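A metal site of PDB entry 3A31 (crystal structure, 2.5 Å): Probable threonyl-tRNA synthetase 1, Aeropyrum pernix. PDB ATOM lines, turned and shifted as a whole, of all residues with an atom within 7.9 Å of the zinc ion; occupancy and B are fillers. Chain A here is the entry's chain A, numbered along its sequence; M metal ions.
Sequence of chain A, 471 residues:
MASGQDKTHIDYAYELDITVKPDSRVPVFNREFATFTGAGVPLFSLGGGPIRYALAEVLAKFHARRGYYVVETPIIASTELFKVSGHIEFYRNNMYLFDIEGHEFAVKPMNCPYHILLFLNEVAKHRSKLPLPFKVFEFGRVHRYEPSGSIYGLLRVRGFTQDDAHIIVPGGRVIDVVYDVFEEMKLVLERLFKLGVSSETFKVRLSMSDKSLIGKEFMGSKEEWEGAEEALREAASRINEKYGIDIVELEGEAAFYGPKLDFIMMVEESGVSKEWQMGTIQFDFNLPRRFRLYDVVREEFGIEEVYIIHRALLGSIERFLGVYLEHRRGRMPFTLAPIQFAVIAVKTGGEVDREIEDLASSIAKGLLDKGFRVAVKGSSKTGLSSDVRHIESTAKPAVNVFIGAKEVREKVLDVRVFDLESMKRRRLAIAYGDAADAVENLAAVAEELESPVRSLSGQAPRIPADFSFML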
ATOM      1  N   MET A 110     -25.927  -6.473 -22.693  1.00  0.00           N
ATOM      2  CA  MET A 110     -26.366  -7.860 -22.395  1.00  0.00           C
ATOM      3  C   MET A 110     -25.448  -8.401 -21.354  1.00  0.00           C
ATOM      4  O   MET A 110     -24.343  -7.854 -21.188  1.00  0.00           O
ATOM      5  CB  MET A 110     -26.271  -8.720 -23.645  1.00  0.00           C
ATOM      6  CG  MET A 110     -24.892  -8.731 -24.337  1.00  0.00           C
ATOM      7  SD  MET A 110     -25.004  -9.625 -26.137  1.00  0.00           S
ATOM      8  CE  MET A 110     -26.984  -9.442 -26.451  1.00  0.00           C
ATOM      9  N   ASN A 111     -25.900  -9.450 -20.666  1.00  0.00           N
ATOM     10  CA  ASN A 111     -25.205 -10.073 -19.508  1.00  0.00           C
ATOM     11  C   ASN A 111     -24.355 -11.279 -19.890  1.00  0.00           C
ATOM     12  O   ASN A 111     -23.414 -11.617 -19.176  1.00  0.00           O
ATOM     13  CB  ASN A 111     -26.213 -10.584 -18.467  1.00  0.00           C
ATOM     14  CG  ASN A 111     -27.041  -9.496 -17.877  1.00  0.00           C
ATOM     15  OD1 ASN A 111     -28.246  -9.535 -17.961  1.00  0.00           O
ATOM     16  ND2 ASN A 111     -26.389  -8.510 -17.293  1.00  0.00           N
ATOM     17  N   CYS A 112     -24.757 -11.937 -20.981  1.00  0.00           N
ATOM     18  CA  CYS A 112     -24.177 -13.222 -21.484  1.00  0.00           C
ATOM     19  C   CYS A 112     -22.636 -13.398 -21.394  1.00  0.00           C
ATOM     20  O   CYS A 112     -22.161 -14.459 -20.908  1.00  0.00           O
ATOM     21  CB  CYS A 112     -24.703 -13.538 -22.923  1.00  0.00           C
ATOM     22  SG  CYS A 112     -26.129 -12.419 -23.523  1.00  0.00           S
ATOM     23  N   PRO A 113     -21.852 -12.420 -21.932  1.00  0.00           N
ATOM     24  CA  PRO A 113     -20.403 -12.470 -21.839  1.00  0.00           C
ATOM     25  C   PRO A 113     -19.897 -12.522 -20.415  1.00  0.00           C
ATOM     26  O   PRO A 113     -18.952 -13.317 -20.114  1.00  0.00           O
ATOM     27  CB  PRO A 113     -19.998 -11.168 -22.527  1.00  0.00           C
ATOM     28  CG  PRO A 113     -21.074 -10.912 -23.557  1.00  0.00           C
ATOM     29  CD  PRO A 113     -22.291 -11.267 -22.761  1.00  0.00           C
ATOM     30  N   HIS A 115     -21.649 -13.622 -17.702  1.00  0.00           N
ATOM     31  CA  HIS A 115     -22.046 -14.939 -17.186  1.00  0.00           C
ATOM     32  C   HIS A 115     -21.137 -16.060 -17.650  1.00  0.00           C
ATOM     33  O   HIS A 115     -20.851 -16.962 -16.863  1.00  0.00           O
ATOM     34  CB  HIS A 115     -23.504 -15.261 -17.516  1.00  0.00           C
ATOM     35  CG  HIS A 115     -24.480 -14.381 -16.796  1.00  0.00           C
ATOM     36  ND1 HIS A 115     -25.839 -14.604 -16.821  1.00  0.00           N
ATOM     37  CD2 HIS A 115     -24.288 -13.295 -15.991  1.00  0.00           C
ATOM     38  CE1 HIS A 115     -26.436 -13.696 -16.072  1.00  0.00           C
ATOM     39  NE2 HIS A 115     -25.516 -12.890 -15.557  1.00  0.00           N
ATOM     40  N   ILE A 116     -20.631 -15.974 -18.894  1.00  0.00           N
ATOM     41  CA  ILE A 116     -19.631 -16.934 -19.391  1.00  0.00           C
ATOM     42  C   ILE A 116     -18.263 -16.753 -18.775  1.00  0.00           C
ATOM     43  O   ILE A 116     -17.607 -17.728 -18.486  1.00  0.00           O
ATOM     44  CB  ILE A 116     -19.507 -16.892 -20.887  1.00  0.00           C
ATOM     45  CG1 ILE A 116     -20.843 -17.354 -21.462  1.00  0.00           C
ATOM     46  CG2 ILE A 116     -18.312 -17.780 -21.400  1.00  0.00           C
ATOM     47  CD1 ILE A 116     -21.034 -16.900 -22.877  1.00  0.00           C
ATOM     48  N   ARG A 144     -29.440  -0.097 -24.186  1.00  0.00           N
ATOM     49  CA  ARG A 144     -29.327  -0.237 -25.613  1.00  0.00           C
ATOM     50  C   ARG A 144     -29.736   1.064 -26.230  1.00  0.00           C
ATOM     51  O   ARG A 144     -30.579   1.794 -25.687  1.00  0.00           O
ATOM     52  CB  ARG A 144     -30.239  -1.364 -26.104  1.00  0.00           C
ATOM     53  CG  ARG A 144     -29.845  -2.660 -25.478  1.00  0.00           C
ATOM     54  CD  ARG A 144     -30.695  -3.811 -25.947  1.00  0.00           C
ATOM     55  NE  ARG A 144     -30.189  -5.032 -25.349  1.00  0.00           N
ATOM     56  CZ  ARG A 144     -30.784  -6.209 -25.405  1.00  0.00           C
ATOM     57  NH1 ARG A 144     -31.938  -6.326 -26.058  1.00  0.00           N
ATOM     58  NH2 ARG A 144     -30.240  -7.247 -24.787  1.00  0.00           N
ATOM     59  N   GLN A 162     -33.791  -7.439 -17.005  1.00  0.00           N
ATOM     60  CA  GLN A 162     -34.235  -8.770 -17.424  1.00  0.00           C
ATOM     61  C   GLN A 162     -34.059  -9.794 -16.295  1.00  0.00           C
ATOM     62  O   GLN A 162     -33.145  -9.674 -15.489  1.00  0.00           O
ATOM     63  CB  GLN A 162     -33.389  -9.279 -18.587  1.00  0.00           C
ATOM     64  CG  GLN A 162     -33.190  -8.342 -19.718  1.00  0.00           C
ATOM     65  CD  GLN A 162     -31.977  -8.727 -20.552  1.00  0.00           C
ATOM     66  OE1 GLN A 162     -30.849  -8.857 -20.054  1.00  0.00           O
ATOM     67  NE2 GLN A 162     -32.204  -8.934 -21.842  1.00  0.00           N
ATOM     68  N   ASP A 164     -32.715 -12.668 -16.454  1.00  0.00           N
ATOM     69  CA  ASP A 164     -31.835 -13.275 -17.401  1.00  0.00           C
ATOM     70  C   ASP A 164     -31.121 -14.519 -16.823  1.00  0.00           C
ATOM     71  O   ASP A 164     -30.717 -14.507 -15.658  1.00  0.00           O
ATOM     72  CB  ASP A 164     -30.821 -12.194 -17.840  1.00  0.00           C
ATOM     73  CG  ASP A 164     -30.154 -12.541 -19.184  1.00  0.00           C
ATOM     74  OD1 ASP A 164     -30.749 -13.372 -19.953  1.00  0.00           O
ATOM     75  OD2 ASP A 164     -29.039 -11.977 -19.446  1.00  0.00           O
ATOM     76  N   ALA A 165     -30.943 -15.584 -17.609  1.00  0.00           N
ATOM     77  CA  ALA A 165     -30.170 -16.743 -17.113  1.00  0.00           C
ATOM     78  C   ALA A 165     -29.384 -17.378 -18.239  1.00  0.00           C
ATOM     79  O   ALA A 165     -29.738 -17.249 -19.410  1.00  0.00           O
ATOM     80  CB  ALA A 165     -31.076 -17.756 -16.428  1.00  0.00           C
ATOM     81  N   HIS A 166     -28.297 -18.026 -17.893  1.00  0.00           N
ATOM     82  CA  HIS A 166     -27.564 -18.790 -18.854  1.00  0.00           C
ATOM     83  C   HIS A 166     -27.341 -20.202 -18.340  1.00  0.00           C
ATOM     84  O   HIS A 166     -27.121 -20.402 -17.114  1.00  0.00           O
ATOM     85  CB  HIS A 166     -26.284 -18.039 -19.320  1.00  0.00           C
ATOM     86  CG  HIS A 166     -26.618 -16.784 -20.076  1.00  0.00           C
ATOM     87  ND1 HIS A 166     -26.780 -15.565 -19.460  1.00  0.00           N
ATOM     88  CD2 HIS A 166     -26.964 -16.582 -21.370  1.00  0.00           C
ATOM     89  CE1 HIS A 166     -27.134 -14.652 -20.339  1.00  0.00           C
ATOM     90  NE2 HIS A 166     -27.239 -15.241 -21.521  1.00  0.00           N
ATOM     91  N   TYR A 257     -27.759 -17.848 -34.912  1.00  0.00           N
ATOM     92  CA  TYR A 257     -26.925 -18.611 -33.961  1.00  0.00           C
ATOM     93  C   TYR A 257     -27.648 -19.711 -33.206  1.00  0.00           C
ATOM     94  O   TYR A 257     -27.023 -20.352 -32.345  1.00  0.00           O
ATOM     95  CB  TYR A 257     -26.237 -17.690 -32.927  1.00  0.00           C
ATOM     96  CG  TYR A 257     -27.195 -16.697 -32.281  1.00  0.00           C
ATOM     97  CD1 TYR A 257     -27.866 -17.014 -31.103  1.00  0.00           C
ATOM     98  CD2 TYR A 257     -27.416 -15.435 -32.860  1.00  0.00           C
ATOM     99  CE1 TYR A 257     -28.715 -16.115 -30.524  1.00  0.00           C
ATOM    100  CE2 TYR A 257     -28.297 -14.513 -32.299  1.00  0.00           C
ATOM    101  CZ  TYR A 257     -28.930 -14.880 -31.134  1.00  0.00           C
ATOM    102  OH  TYR A 257     -29.826 -13.995 -30.609  1.00  0.00           O
ATOM    103  N   GLN A 282     -33.402 -19.475 -26.025  1.00  0.00           N
ATOM    104  CA  GLN A 282     -32.523 -19.271 -27.179  1.00  0.00           C
ATOM    105  C   GLN A 282     -31.245 -20.107 -27.055  1.00  0.00           C
ATOM    106  O   GLN A 282     -30.405 -19.862 -26.191  1.00  0.00           O
ATOM    107  CB  GLN A 282     -32.134 -17.767 -27.227  1.00  0.00           C
ATOM    108  CG  GLN A 282     -31.217 -17.401 -28.349  1.00  0.00           C
ATOM    109  CD  GLN A 282     -31.893 -17.637 -29.687  1.00  0.00           C
ATOM    110  OE1 GLN A 282     -32.906 -16.999 -29.978  1.00  0.00           O
ATOM    111  NE2 GLN A 282     -31.368 -18.573 -30.489  1.00  0.00           N
ATOM    112  N   ASP A 284     -27.558 -21.119 -28.528  1.00  0.00           N
ATOM    113  CA  ASP A 284     -26.499 -20.311 -29.095  1.00  0.00           C
ATOM    114  C   ASP A 284     -25.311 -21.197 -29.542  1.00  0.00           C
ATOM    115  O   ASP A 284     -24.714 -21.907 -28.707  1.00  0.00           O
ATOM    116  CB  ASP A 284     -26.043 -19.294 -28.044  1.00  0.00           C
ATOM    117  CG  ASP A 284     -25.212 -18.185 -28.610  1.00  0.00           C
ATOM    118  OD1 ASP A 284     -24.293 -18.458 -29.456  1.00  0.00           O
ATOM    119  OD2 ASP A 284     -25.471 -17.002 -28.196  1.00  0.00           O
ATOM    120  N   LEU A 287     -21.552 -18.397 -29.182  1.00  0.00           N
ATOM    121  CA  LEU A 287     -20.800 -18.214 -27.917  1.00  0.00           C
ATOM    122  C   LEU A 287     -19.880 -19.387 -27.601  1.00  0.00           C
ATOM    123  O   LEU A 287     -18.748 -19.165 -27.207  1.00  0.00           O
ATOM    124  CB  LEU A 287     -21.734 -17.971 -26.712  1.00  0.00           C
ATOM    125  CG  LEU A 287     -22.487 -16.668 -26.657  1.00  0.00           C
ATOM    126  CD1 LEU A 287     -23.501 -16.662 -25.536  1.00  0.00           C
ATOM    127  CD2 LEU A 287     -21.522 -15.457 -26.600  1.00  0.00           C
ATOM    128  N   ILE A 308     -25.512 -24.359 -25.115  1.00  0.00           N
ATOM    129  CA  ILE A 308     -25.496 -23.080 -24.410  1.00  0.00           C
ATOM    130  C   ILE A 308     -26.873 -22.396 -24.624  1.00  0.00           C
ATOM    131  O   ILE A 308     -27.398 -22.312 -25.743  1.00  0.00           O
ATOM    132  CB  ILE A 308     -24.386 -22.119 -24.931  1.00  0.00           C
ATOM    133  CG1 ILE A 308     -23.011 -22.426 -24.331  1.00  0.00           C
ATOM    134  CG2 ILE A 308     -24.657 -20.748 -24.457  1.00  0.00           C
ATOM    135  CD1 ILE A 308     -22.361 -23.699 -24.809  1.00  0.00           C
ATOM    136  N   ILE A 309     -27.442 -21.864 -23.558  1.00  0.00           N
ATOM    137  CA  ILE A 309     -28.799 -21.396 -23.666  1.00  0.00           C
ATOM    138  C   ILE A 309     -28.960 -20.069 -22.943  1.00  0.00           C
ATOM    139  O   ILE A 309     -28.459 -19.928 -21.816  1.00  0.00           O
ATOM    140  CB  ILE A 309     -29.788 -22.469 -23.078  1.00  0.00           C
ATOM    141  CG1 ILE A 309     -29.762 -23.734 -23.941  1.00  0.00           C
ATOM    142  CG2 ILE A 309     -31.171 -21.888 -22.896  1.00  0.00           C
ATOM    143  CD1 ILE A 309     -30.788 -24.810 -23.546  1.00  0.00           C
ATOM    144  N   HIS A 310     -29.648 -19.116 -23.590  1.00  0.00           N
ATOM    145  CA  HIS A 310     -30.098 -17.829 -22.973  1.00  0.00           C
ATOM    146  C   HIS A 310     -31.573 -18.100 -22.675  1.00  0.00           C
ATOM    147  O   HIS A 310     -32.283 -18.676 -23.542  1.00  0.00           O
ATOM    148  CB  HIS A 310     -30.094 -16.650 -23.942  1.00  0.00           C
ATOM    149  CG  HIS A 310     -28.825 -16.435 -24.708  1.00  0.00           C
ATOM    150  ND1 HIS A 310     -28.001 -15.343 -24.509  1.00  0.00           N
ATOM    151  CD2 HIS A 310     -28.279 -17.127 -25.738  1.00  0.00           C
ATOM    152  CE1 HIS A 310     -26.990 -15.392 -25.355  1.00  0.00           C
ATOM    153  NE2 HIS A 310     -27.139 -16.457 -26.116  1.00  0.00           N
ATOM    154  N   ARG A 311     -32.050 -17.715 -21.475  1.00  0.00           N
ATOM    155  CA  ARG A 311     -33.500 -17.742 -21.193  1.00  0.00           C
ATOM    156  C   ARG A 311     -33.940 -16.613 -20.293  1.00  0.00           C
ATOM    157  O   ARG A 311     -33.177 -16.201 -19.413  1.00  0.00           O
ATOM    158  CB  ARG A 311     -33.951 -19.112 -20.639  1.00  0.00           C
ATOM    159  CG  ARG A 311     -33.091 -19.724 -19.535  1.00  0.00           C
ATOM    160  CD  ARG A 311     -33.799 -19.641 -18.200  1.00  0.00           C
ATOM    161  NE  ARG A 311     -34.001 -18.284 -17.664  1.00  0.00           N
ATOM    162  CZ  ARG A 311     -34.625 -18.010 -16.528  1.00  0.00           C
ATOM    163  NH1 ARG A 311     -35.128 -19.012 -15.754  1.00  0.00           N
ATOM    164  NH2 ARG A 311     -34.746 -16.747 -16.148  1.00  0.00           N
HETATM  165 ZN    ZN M   1     -27.811 -14.051 -22.997  1.00  0.00          ZN
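ND1 of His 166 is in hydrogen-bond range of ND1 of His 115 (3.0 Å). A ring nitrogen (NE2) of His 310 is in hydrogen-bond range of the side-chain carboxylate of Asp 284 (2.7 Å). The backbone NH (N) of His 310 lies within hydrogen-bond range of the backbone carbonyl oxygen (O) of Gln 282 (2.8 Å).
The zinc ion is bound by NE2 of His 166 (2.0 Å), ND1 of His 310 (2.0 Å) and SG of Cys 112 (2.4 Å).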
